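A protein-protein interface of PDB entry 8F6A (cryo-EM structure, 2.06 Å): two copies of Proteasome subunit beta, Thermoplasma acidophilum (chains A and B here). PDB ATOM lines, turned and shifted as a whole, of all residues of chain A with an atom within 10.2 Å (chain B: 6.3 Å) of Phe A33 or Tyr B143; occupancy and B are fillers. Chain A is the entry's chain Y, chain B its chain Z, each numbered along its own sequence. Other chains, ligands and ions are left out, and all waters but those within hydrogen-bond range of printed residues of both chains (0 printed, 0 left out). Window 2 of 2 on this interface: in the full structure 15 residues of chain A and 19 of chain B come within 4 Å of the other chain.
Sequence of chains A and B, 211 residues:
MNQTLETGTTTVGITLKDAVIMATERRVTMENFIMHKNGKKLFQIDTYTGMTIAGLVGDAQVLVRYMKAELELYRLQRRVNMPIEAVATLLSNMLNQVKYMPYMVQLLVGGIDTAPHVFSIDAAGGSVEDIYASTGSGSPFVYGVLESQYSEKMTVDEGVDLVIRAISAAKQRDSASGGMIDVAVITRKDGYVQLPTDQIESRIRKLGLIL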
ATOM      1  N   ARG A  26     -19.546  -3.334 -37.636  1.00  0.00           N
ATOM      2  CA  ARG A  26     -18.908  -4.637 -37.477  1.00  0.00           C
ATOM      3  C   ARG A  26     -18.736  -5.117 -36.035  1.00  0.00           C
ATOM      4  O   ARG A  26     -18.117  -6.169 -35.829  1.00  0.00           O
ATOM      5  CB  ARG A  26     -17.531  -4.621 -38.150  1.00  0.00           C
ATOM      6  CG  ARG A  26     -17.564  -4.544 -39.662  1.00  0.00           C
ATOM      7  CD  ARG A  26     -16.342  -5.214 -40.262  1.00  0.00           C
ATOM      8  NE  ARG A  26     -15.968  -4.635 -41.546  1.00  0.00           N
ATOM      9  CZ  ARG A  26     -14.729  -4.593 -42.016  1.00  0.00           C
ATOM     10  NH1 ARG A  26     -13.712  -5.088 -41.332  1.00  0.00           N
ATOM     11  NH2 ARG A  26     -14.506  -4.034 -43.202  1.00  0.00           N
ATOM     12  N   ARG A  27     -19.254  -4.412 -35.035  1.00  0.00           N
ATOM     13  CA  ARG A  27     -18.982  -4.777 -33.648  1.00  0.00           C
ATOM     14  C   ARG A  27     -19.892  -5.923 -33.210  1.00  0.00           C
ATOM     15  O   ARG A  27     -21.110  -5.861 -33.387  1.00  0.00           O
ATOM     16  CB  ARG A  27     -19.157  -3.564 -32.731  1.00  0.00           C
ATOM     17  CG  ARG A  27     -19.335  -3.904 -31.256  1.00  0.00           C
ATOM     18  CD  ARG A  27     -19.027  -2.722 -30.329  1.00  0.00           C
ATOM     19  NE  ARG A  27     -17.924  -1.886 -30.785  1.00  0.00           N
ATOM     20  CZ  ARG A  27     -17.639  -0.686 -30.294  1.00  0.00           C
ATOM     21  NH1 ARG A  27     -18.385  -0.130 -29.354  1.00  0.00           N
ATOM     22  NH2 ARG A  27     -16.577  -0.032 -30.752  1.00  0.00           N
ATOM     23  N   VAL A  28     -19.296  -6.970 -32.639  1.00  0.00           N
ATOM     24  CA  VAL A  28     -20.052  -8.133 -32.176  1.00  0.00           C
ATOM     25  C   VAL A  28     -19.858  -8.325 -30.678  1.00  0.00           C
ATOM     26  O   VAL A  28     -18.818  -8.816 -30.236  1.00  0.00           O
ATOM     27  CB  VAL A  28     -19.647  -9.407 -32.939  1.00  0.00           C
ATOM     28  CG1 VAL A  28     -20.384 -10.616 -32.379  1.00  0.00           C
ATOM     29  CG2 VAL A  28     -19.919  -9.252 -34.427  1.00  0.00           C
ATOM     30  N   THR A  29     -20.857  -7.966 -29.887  1.00  0.00           N
ATOM     31  CA  THR A  29     -20.765  -8.167 -28.447  1.00  0.00           C
ATOM     32  C   THR A  29     -20.982  -9.635 -28.104  1.00  0.00           C
ATOM     33  O   THR A  29     -21.924 -10.264 -28.592  1.00  0.00           O
ATOM     34  CB  THR A  29     -21.792  -7.287 -27.731  1.00  0.00           C
ATOM     35  OG1 THR A  29     -21.385  -5.917 -27.816  1.00  0.00           O
ATOM     36  CG2 THR A  29     -21.909  -7.680 -26.265  1.00  0.00           C
ATOM     37  N   MET A  30     -20.092 -10.190 -27.286  1.00  0.00           N
ATOM     38  CA  MET A  30     -20.249 -11.542 -26.773  1.00  0.00           C
ATOM     39  C   MET A  30     -19.602 -11.623 -25.395  1.00  0.00           C
ATOM     40  O   MET A  30     -18.561 -11.009 -25.148  1.00  0.00           O
ATOM     41  CB  MET A  30     -19.656 -12.577 -27.751  1.00  0.00           C
ATOM     42  CG  MET A  30     -20.016 -14.016 -27.433  1.00  0.00           C
ATOM     43  SD  MET A  30     -19.480 -15.218 -28.664  1.00  0.00           S
ATOM     44  CE  MET A  30     -17.853 -14.653 -29.081  1.00  0.00           C
ATOM     45  N   GLU A  31     -20.245 -12.371 -24.495  1.00  0.00           N
ATOM     46  CA  GLU A  31     -19.857 -12.437 -23.081  1.00  0.00           C
ATOM     47  C   GLU A  31     -19.859 -11.053 -22.432  1.00  0.00           C
ATOM     48  O   GLU A  31     -19.053 -10.755 -21.550  1.00  0.00           O
ATOM     49  CB  GLU A  31     -18.497 -13.118 -22.906  1.00  0.00           C
ATOM     50  CG  GLU A  31     -18.505 -14.614 -23.171  1.00  0.00           C
ATOM     51  CD  GLU A  31     -19.183 -15.407 -22.065  1.00  0.00           C
ATOM     52  OE1 GLU A  31     -19.824 -16.431 -22.376  1.00  0.00           O
ATOM     53  OE2 GLU A  31     -19.069 -15.015 -20.887  1.00  0.00           O
ATOM     54  N   ASN A  32     -20.783 -10.202 -22.880  1.00  0.00           N
ATOM     55  CA  ASN A  32     -21.017  -8.879 -22.294  1.00  0.00           C
ATOM     56  C   ASN A  32     -19.775  -7.984 -22.341  1.00  0.00           C
ATOM     57  O   ASN A  32     -19.501  -7.217 -21.418  1.00  0.00           O
ATOM     58  CB  ASN A  32     -21.541  -9.008 -20.862  1.00  0.00           C
ATOM     59  CG  ASN A  32     -22.745  -9.925 -20.763  1.00  0.00           C
ATOM     60  OD1 ASN A  32     -22.610 -11.150 -20.769  1.00  0.00           O
ATOM     61  ND2 ASN A  32     -23.930  -9.337 -20.679  1.00  0.00           N
ATOM     62  N   PHE A  33     -19.027  -8.076 -23.439  1.00  0.00           N
ATOM     63  CA  PHE A  33     -17.928  -7.153 -23.691  1.00  0.00           C
ATOM     64  C   PHE A  33     -17.639  -7.157 -25.184  1.00  0.00           C
ATOM     65  O   PHE A  33     -18.205  -7.953 -25.936  1.00  0.00           O
ATOM     66  CB  PHE A  33     -16.680  -7.501 -22.861  1.00  0.00           C
ATOM     67  CG  PHE A  33     -15.849  -8.616 -23.428  1.00  0.00           C
ATOM     68  CD1 PHE A  33     -16.231  -9.939 -23.261  1.00  0.00           C
ATOM     69  CD2 PHE A  33     -14.675  -8.347 -24.116  1.00  0.00           C
ATOM     70  CE1 PHE A  33     -15.465 -10.970 -23.773  1.00  0.00           C
ATOM     71  CE2 PHE A  33     -13.901  -9.376 -24.628  1.00  0.00           C
ATOM     72  CZ  PHE A  33     -14.298 -10.689 -24.458  1.00  0.00           C
ATOM     73  N   ILE A  34     -16.749  -6.260 -25.608  1.00  0.00           N
ATOM     74  CA  ILE A  34     -16.476  -6.130 -27.033  1.00  0.00           C
ATOM     75  C   ILE A  34     -15.423  -7.152 -27.441  1.00  0.00           C
ATOM     76  O   ILE A  34     -14.236  -6.842 -27.555  1.00  0.00           O
ATOM     77  CB  ILE A  34     -16.027  -4.703 -27.400  1.00  0.00           C
ATOM     78  CG1 ILE A  34     -17.006  -3.667 -26.843  1.00  0.00           C
ATOM     79  CG2 ILE A  34     -15.903  -4.555 -28.909  1.00  0.00           C
ATOM     80  CD1 ILE A  34     -16.573  -2.248 -27.075  1.00  0.00           C
ATOM     81  N   MET A  35     -15.869  -8.393 -27.663  1.00  0.00           N
ATOM     82  CA  MET A  35     -14.920  -9.498 -27.975  1.00  0.00           C
ATOM     83  C   MET A  35     -14.415  -9.399 -29.416  1.00  0.00           C
ATOM     84  O   MET A  35     -13.204  -9.583 -29.625  1.00  0.00           O
ATOM     85  CB  MET A  35     -15.601 -10.857 -27.784  1.00  0.00           C
ATOM     86  CG  MET A  35     -14.668 -12.031 -27.998  1.00  0.00           C
ATOM     87  SD  MET A  35     -15.242 -13.529 -27.164  1.00  0.00           S
ATOM     88  CE  MET A  35     -13.850 -14.620 -27.455  1.00  0.00           C
ATOM     89  N   HIS A  36     -15.308  -9.152 -30.375  1.00  0.00           N
ATOM     90  CA  HIS A  36     -14.892  -9.132 -31.802  1.00  0.00           C
ATOM     91  C   HIS A  36     -15.190  -7.753 -32.395  1.00  0.00           C
ATOM     92  O   HIS A  36     -16.380  -7.393 -32.516  1.00  0.00           O
ATOM     93  CB  HIS A  36     -15.596 -10.249 -32.575  1.00  0.00           C
ATOM     94  CG  HIS A  36     -15.397 -11.600 -31.979  1.00  0.00           C
ATOM     95  ND1 HIS A  36     -14.234 -12.322 -32.148  1.00  0.00           N
ATOM     96  CD2 HIS A  36     -16.196 -12.358 -31.221  1.00  0.00           C
ATOM     97  CE1 HIS A  36     -14.341 -13.475 -31.509  1.00  0.00           C
ATOM     98  NE2 HIS A  36     -15.522 -13.519 -30.939  1.00  0.00           N
ATOM     99  N   LYS A  37     -14.108  -6.998 -32.759  1.00  0.00           N
ATOM    100  CA  LYS A  37     -14.385  -5.710 -33.383  1.00  0.00           C
ATOM    101  C   LYS A  37     -14.620  -5.786 -34.893  1.00  0.00           C
ATOM    102  O   LYS A  37     -14.909  -4.756 -35.503  1.00  0.00           O
ATOM    103  CB  LYS A  37     -13.235  -4.734 -33.099  1.00  0.00           C
ATOM    104  CG  LYS A  37     -12.686  -4.815 -31.686  1.00  0.00           C
ATOM    105  CD  LYS A  37     -11.167  -4.688 -31.661  1.00  0.00           C
ATOM    106  CE  LYS A  37     -10.698  -3.855 -30.478  1.00  0.00           C
ATOM    107  NZ  LYS A  37      -9.220  -3.663 -30.469  1.00  0.00           N
ATOM    108  N   VAL A  57     -26.432 -13.948 -32.802  1.00  0.00           N
ATOM    109  CA  VAL A  57     -25.481 -14.244 -33.874  1.00  0.00           C
ATOM    110  C   VAL A  57     -25.689 -15.660 -34.399  1.00  0.00           C
ATOM    111  O   VAL A  57     -25.749 -15.890 -35.613  1.00  0.00           O
ATOM    112  CB  VAL A  57     -24.037 -14.033 -33.390  1.00  0.00           C
ATOM    113  CG1 VAL A  57     -23.050 -14.377 -34.495  1.00  0.00           C
ATOM    114  CG2 VAL A  57     -23.842 -12.600 -32.926  1.00  0.00           C
ATOM    115  N   SER A 175     -23.668   2.323 -27.917  1.00  0.00           N
ATOM    116  CA  SER A 175     -22.450   1.632 -27.500  1.00  0.00           C
ATOM    117  C   SER A 175     -22.354   0.230 -28.091  1.00  0.00           C
ATOM    118  O   SER A 175     -21.251  -0.306 -28.232  1.00  0.00           O
ATOM    119  CB  SER A 175     -22.380   1.579 -25.973  1.00  0.00           C
ATOM    120  OG  SER A 175     -23.162   0.515 -25.464  1.00  0.00           O
ATOM    121  N   ALA A 176     -23.487  -0.377 -28.447  1.00  0.00           N
ATOM    122  CA  ALA A 176     -23.469  -1.705 -29.051  1.00  0.00           C
ATOM    123  C   ALA A 176     -22.948  -1.704 -30.486  1.00  0.00           C
ATOM    124  O   ALA A 176     -22.708  -2.783 -31.033  1.00  0.00           O
ATOM    125  CB  ALA A 176     -24.868  -2.322 -29.011  1.00  0.00           C
ATOM    126  N   SER A 177     -22.769  -0.541 -31.101  1.00  0.00           N
ATOM    127  CA  SER A 177     -22.291  -0.442 -32.472  1.00  0.00           C
ATOM    128  C   SER A 177     -20.856   0.069 -32.498  1.00  0.00           C
ATOM    129  O   SER A 177     -20.393   0.727 -31.563  1.00  0.00           O
ATOM    130  CB  SER A 177     -23.194   0.485 -33.298  1.00  0.00           C
ATOM    131  OG  SER A 177     -24.520  -0.011 -33.357  1.00  0.00           O
ATOM    132  N   ASP B 130     -11.504 -14.352 -35.522  1.00  0.00           N
ATOM    133  CA  ASP B 130     -10.778 -13.226 -34.947  1.00  0.00           C
ATOM    134  C   ASP B 130      -9.281 -13.502 -34.999  1.00  0.00           C
ATOM    135  O   ASP B 130      -8.845 -14.651 -35.102  1.00  0.00           O
ATOM    136  CB  ASP B 130     -11.215 -12.952 -33.505  1.00  0.00           C
ATOM    137  CG  ASP B 130     -11.103 -11.485 -33.130  1.00  0.00           C
ATOM    138  OD1 ASP B 130     -10.044 -10.876 -33.381  1.00  0.00           O
ATOM    139  OD2 ASP B 130     -12.079 -10.939 -32.582  1.00  0.00           O
ATOM    140  N   TYR B 132      -7.275 -12.822 -32.456  1.00  0.00           N
ATOM    141  CA  TYR B 132      -7.061 -13.480 -31.173  1.00  0.00           C
ATOM    142  C   TYR B 132      -8.366 -13.470 -30.388  1.00  0.00           C
ATOM    143  O   TYR B 132      -9.273 -12.683 -30.670  1.00  0.00           O
ATOM    144  CB  TYR B 132      -5.925 -12.831 -30.361  1.00  0.00           C
ATOM    145  CG  TYR B 132      -6.108 -11.368 -29.998  1.00  0.00           C
ATOM    146  CD1 TYR B 132      -7.015 -10.975 -29.019  1.00  0.00           C
ATOM    147  CD2 TYR B 132      -5.343 -10.380 -30.611  1.00  0.00           C
ATOM    148  CE1 TYR B 132      -7.172  -9.644 -28.681  1.00  0.00           C
ATOM    149  CE2 TYR B 132      -5.492  -9.049 -30.277  1.00  0.00           C
ATOM    150  CZ  TYR B 132      -6.409  -8.686 -29.310  1.00  0.00           C
ATOM    151  OH  TYR B 132      -6.564  -7.362 -28.976  1.00  0.00           O
ATOM    152  N   ALA B 133      -8.452 -14.359 -29.400  1.00  0.00           N
ATOM    153  CA  ALA B 133      -9.647 -14.469 -28.571  1.00  0.00           C
ATOM    154  C   ALA B 133      -9.298 -15.169 -27.264  1.00  0.00           C
ATOM    155  O   ALA B 133      -8.274 -15.847 -27.154  1.00  0.00           O
ATOM    156  CB  ALA B 133     -10.770 -15.216 -29.299  1.00  0.00           C
ATOM    157  N   SER B 134     -10.174 -15.001 -26.273  1.00  0.00           N
ATOM    158  CA  SER B 134      -9.984 -15.598 -24.959  1.00  0.00           C
ATOM    159  C   SER B 134     -11.340 -15.894 -24.335  1.00  0.00           C
ATOM    160  O   SER B 134     -12.285 -15.120 -24.500  1.00  0.00           O
ATOM    161  CB  SER B 134      -9.162 -14.678 -24.046  1.00  0.00           C
ATOM    162  OG  SER B 134      -8.858 -15.312 -22.819  1.00  0.00           O
ATOM    163  N   THR B 135     -11.427 -17.011 -23.614  1.00  0.00           N
ATOM    164  CA  THR B 135     -12.662 -17.450 -22.975  1.00  0.00           C
ATOM    165  C   THR B 135     -12.404 -17.774 -21.509  1.00  0.00           C
ATOM    166  O   THR B 135     -11.262 -17.824 -21.048  1.00  0.00           O
ATOM    167  CB  THR B 135     -13.267 -18.677 -23.677  1.00  0.00           C
ATOM    168  OG1 THR B 135     -12.373 -19.790 -23.553  1.00  0.00           O
ATOM    169  CG2 THR B 135     -13.526 -18.392 -25.149  1.00  0.00           C
ATOM    170  N   GLY B 138     -11.331 -15.811 -16.535  1.00  0.00           N
ATOM    171  CA  GLY B 138     -10.131 -14.999 -16.580  1.00  0.00           C
ATOM    172  C   GLY B 138      -9.904 -14.230 -17.865  1.00  0.00           C
ATOM    173  O   GLY B 138      -8.925 -13.484 -17.964  1.00  0.00           O
ATOM    174  N   SER B 139     -10.793 -14.385 -18.846  1.00  0.00           N
ATOM    175  CA  SER B 139     -10.609 -13.766 -20.159  1.00  0.00           C
ATOM    176  C   SER B 139     -10.498 -12.242 -20.135  1.00  0.00           C
ATOM    177  O   SER B 139      -9.661 -11.707 -20.879  1.00  0.00           O
ATOM    178  CB  SER B 139     -11.731 -14.231 -21.102  1.00  0.00           C
ATOM    179  OG  SER B 139     -12.912 -13.467 -20.951  1.00  0.00           O
ATOM    180  N   PRO B 140     -11.287 -11.486 -19.353  1.00  0.00           N
ATOM    181  CA  PRO B 140     -11.139 -10.016 -19.401  1.00  0.00           C
ATOM    182  C   PRO B 140      -9.739  -9.538 -19.048  1.00  0.00           C
ATOM    183  O   PRO B 140      -9.239  -8.583 -19.652  1.00  0.00           O
ATOM    184  CB  PRO B 140     -12.188  -9.526 -18.392  1.00  0.00           C
ATOM    185  CG  PRO B 140     -13.149 -10.642 -18.253  1.00  0.00           C
ATOM    186  CD  PRO B 140     -12.336 -11.881 -18.392  1.00  0.00           C
ATOM    187  N   PHE B 141      -9.087 -10.192 -18.084  1.00  0.00           N
ATOM    188  CA  PHE B 141      -7.708  -9.850 -17.759  1.00  0.00           C
ATOM    189  C   PHE B 141      -6.780 -10.151 -18.932  1.00  0.00           C
ATOM    190  O   PHE B 141      -5.821  -9.411 -19.181  1.00  0.00           O
ATOM    191  CB  PHE B 141      -7.271 -10.599 -16.499  1.00  0.00           C
ATOM    192  CG  PHE B 141      -8.248 -10.479 -15.359  1.00  0.00           C
ATOM    193  CD1 PHE B 141      -8.344  -9.303 -14.633  1.00  0.00           C
ATOM    194  CD2 PHE B 141      -9.093 -11.531 -15.038  1.00  0.00           C
ATOM    195  CE1 PHE B 141      -9.247  -9.184 -13.593  1.00  0.00           C
ATOM    196  CE2 PHE B 141     -10.001 -11.417 -13.996  1.00  0.00           C
ATOM    197  CZ  PHE B 141     -10.078 -10.243 -13.274  1.00  0.00           C
ATOM    198  N   VAL B 142      -7.053 -11.232 -19.663  1.00  0.00           N
ATOM    199  CA  VAL B 142      -6.240 -11.577 -20.826  1.00  0.00           C
ATOM    200  C   VAL B 142      -6.376 -10.517 -21.914  1.00  0.00           C
ATOM    201  O   VAL B 142      -5.387 -10.127 -22.543  1.00  0.00           O
ATOM    202  CB  VAL B 142      -6.617 -12.979 -21.339  1.00  0.00           C
ATOM    203  CG1 VAL B 142      -6.042 -13.221 -22.729  1.00  0.00           C
ATOM    204  CG2 VAL B 142      -6.148 -14.049 -20.362  1.00  0.00           C
ATOM    205  N   TYR B 143      -7.598 -10.036 -22.155  1.00  0.00           N
ATOM    206  CA  TYR B 143      -7.804  -9.049 -23.211  1.00  0.00           C
ATOM    207  C   TYR B 143      -7.053  -7.754 -22.916  1.00  0.00           C
ATOM    208  O   TYR B 143      -6.559  -7.096 -23.836  1.00  0.00           O
ATOM    209  CB  TYR B 143      -9.295  -8.781 -23.406  1.00  0.00           C
ATOM    210  CG  TYR B 143      -9.959  -9.763 -24.344  1.00  0.00           C
ATOM    211  CD1 TYR B 143      -9.873  -9.606 -25.723  1.00  0.00           C
ATOM    212  CD2 TYR B 143     -10.672 -10.848 -23.851  1.00  0.00           C
ATOM    213  CE1 TYR B 143     -10.472 -10.508 -26.583  1.00  0.00           C
ATOM    214  CE2 TYR B 143     -11.276 -11.752 -24.700  1.00  0.00           C
ATOM    215  CZ  TYR B 143     -11.176 -11.579 -26.063  1.00  0.00           C
ATOM    216  OH  TYR B 143     -11.777 -12.479 -26.905  1.00  0.00           O
ATOM    217  N   GLY B 144      -6.947  -7.381 -21.639  1.00  0.00           N
ATOM    218  CA  GLY B 144      -6.150  -6.217 -21.289  1.00  0.00           C
ATOM    219  C   GLY B 144      -4.696  -6.371 -21.689  1.00  0.00           C
ATOM    220  O   GLY B 144      -4.092  -5.453 -22.248  1.00  0.00           O
ATOM    221  N   VAL B 145      -4.120  -7.544 -21.422  1.00  0.00           N
ATOM    222  CA  VAL B 145      -2.734  -7.802 -21.807  1.00  0.00           C
ATOM    223  C   VAL B 145      -2.595  -7.803 -23.326  1.00  0.00           C
ATOM    224  O   VAL B 145      -1.686  -7.178 -23.884  1.00  0.00           O
ATOM    225  CB  VAL B 145      -2.246  -9.127 -21.193  1.00  0.00           C
ATOM    226  CG1 VAL B 145      -0.867  -9.491 -21.728  1.00  0.00           C
ATOM    227  CG2 VAL B 145      -2.235  -9.040 -19.668  1.00  0.00           C
ATOM    228  N   LEU B 146      -3.502  -8.498 -24.018  1.00  0.00           N
ATOM    229  CA  LEU B 146      -3.411  -8.607 -25.472  1.00  0.00           C
ATOM    230  C   LEU B 146      -3.598  -7.252 -26.146  1.00  0.00           C
ATOM    231  O   LEU B 146      -2.887  -6.921 -27.100  1.00  0.00           O
ATOM    232  CB  LEU B 146      -4.436  -9.619 -25.985  1.00  0.00           C
ATOM    233  CG  LEU B 146      -4.209 -11.070 -25.553  1.00  0.00           C
ATOM    234  CD1 LEU B 146      -5.198 -12.000 -26.235  1.00  0.00           C
ATOM    235  CD2 LEU B 146      -2.776 -11.512 -25.830  1.00  0.00           C
ATOM    236  N   GLU B 147      -4.543  -6.447 -25.657  1.00  0.00           N
ATOM    237  CA  GLU B 147      -4.781  -5.136 -26.253  1.00  0.00           C
ATOM    238  C   GLU B 147      -3.543  -4.251 -26.208  1.00  0.00           C
ATOM    239  O   GLU B 147      -3.271  -3.537 -27.178  1.00  0.00           O
ATOM    240  CB  GLU B 147      -5.941  -4.430 -25.550  1.00  0.00           C
ATOM    241  CG  GLU B 147      -7.311  -4.820 -26.075  1.00  0.00           C
ATOM    242  CD  GLU B 147      -7.650  -4.137 -27.387  1.00  0.00           C
ATOM    243  OE1 GLU B 147      -8.655  -4.524 -28.012  1.00  0.00           O
ATOM    244  OE2 GLU B 147      -6.919  -3.209 -27.786  1.00  0.00           O
ATOM    245  N   SER B 148      -2.774  -4.294 -25.119  1.00  0.00           N
ATOM    246  CA  SER B 148      -1.613  -3.429 -24.973  1.00  0.00           C
ATOM    247  C   SER B 148      -0.326  -4.005 -25.544  1.00  0.00           C
ATOM    248  O   SER B 148       0.581  -3.231 -25.860  1.00  0.00           O
ATOM    249  CB  SER B 148      -1.382  -3.088 -23.492  1.00  0.00           C
ATOM    250  OG  SER B 148      -1.215  -4.256 -22.715  1.00  0.00           O
ATOM    251  N   ALA B 166      -0.090 -13.357 -20.375  1.00  0.00           N
ATOM    252  CA  ALA B 166      -1.513 -13.047 -20.278  1.00  0.00           C
ATOM    253  C   ALA B 166      -2.217 -13.978 -19.297  1.00  0.00           C
ATOM    254  O   ALA B 166      -3.005 -13.532 -18.457  1.00  0.00           O
ATOM    255  CB  ALA B 166      -2.162 -13.120 -21.659  1.00  0.00           C
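A ring nitrogen (ND1) of His A36 sits at hydrogen-bond distance from the side-chain carboxylate (OD2) of Asp B130, 2.6 Å away.
The side-chain carboxylate (OE1) of Glu B147 is in salt-bridge range of the side-chain amino group (NZ) of Lys A37, 2.7 Å away.
SD of Met A35 lies close to OH of Tyr B143.
The side-chain carboxylate (OD2) of Asp B130 sits close to the backbone carbonyl oxygen (O) of Met A35.
The side-chain sulfur of Met A35 sits close to a ring nitrogen (NE2) of His A36.
O of His A36 sits at hydrogen-bond distance from N of Val A28 (2.9 Å).
The backbone NH of Ser B134 lies within hydrogen-bond range of the side-chain hydroxyl of Tyr B143 (3.1 Å).
Among the printed residues, pairs that only touch across the chains: Phe A33 with Tyr B143 (3.2 Å), Met A35 with Ser B134 (3.4 Å) and Met A35 with Ala B133 (3.6 Å).
Of the printed residues of chain B, Phe A33 touches Tyr B143.
Tyr B143 touches just these residues of chain A: Phe A33 (3.2 Å) and Met A35 (3.0 Å).
Ala B133 touches one residue of chain A.
Ser B134 touches one residue of chain A.
No residue of chain A comes within 4 Å of Ser B139.
No residue of chain A comes within 4 Å of Pro B140.
No residue of chain A comes within 4 Å of Gly B144.
No residue of chain A comes within 4 Å of Leu B146.
Printed residues of chain B within 4 Å of His A36: Asp B130.
Of the printed residues of chain B, Met A35 touches Asp B130, Ala B133, Ser B134 and Tyr B143.
Printed residues of chain A within 4 Å of Asp B130: Met A35 and His A36.
The nearest residue of chain B that does not touch Phe A33 is Ser B139 (4.6 Å).
The nearest printed residue of chain A that does not touch Tyr B143 is Ile A34 (5.3 Å).
The nearest printed residue of chain A that does not touch Asp B130 is Lys A37 (4.4 Å).
Of the 16 printed residues of chain A, 4 touch a printed residue of chain B.
Hydrophobic or aromatic side chains of chain A within 4 Å of the printed part of chain B: Phe A33, Met A35 and His A36.
Among the printed residues, 7 pairs touch across the chains.
No position is printed for both chains.
Of the 7 pairs that touch across the chains among the printed residues, none has its exchanged pair printed and touching as well.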
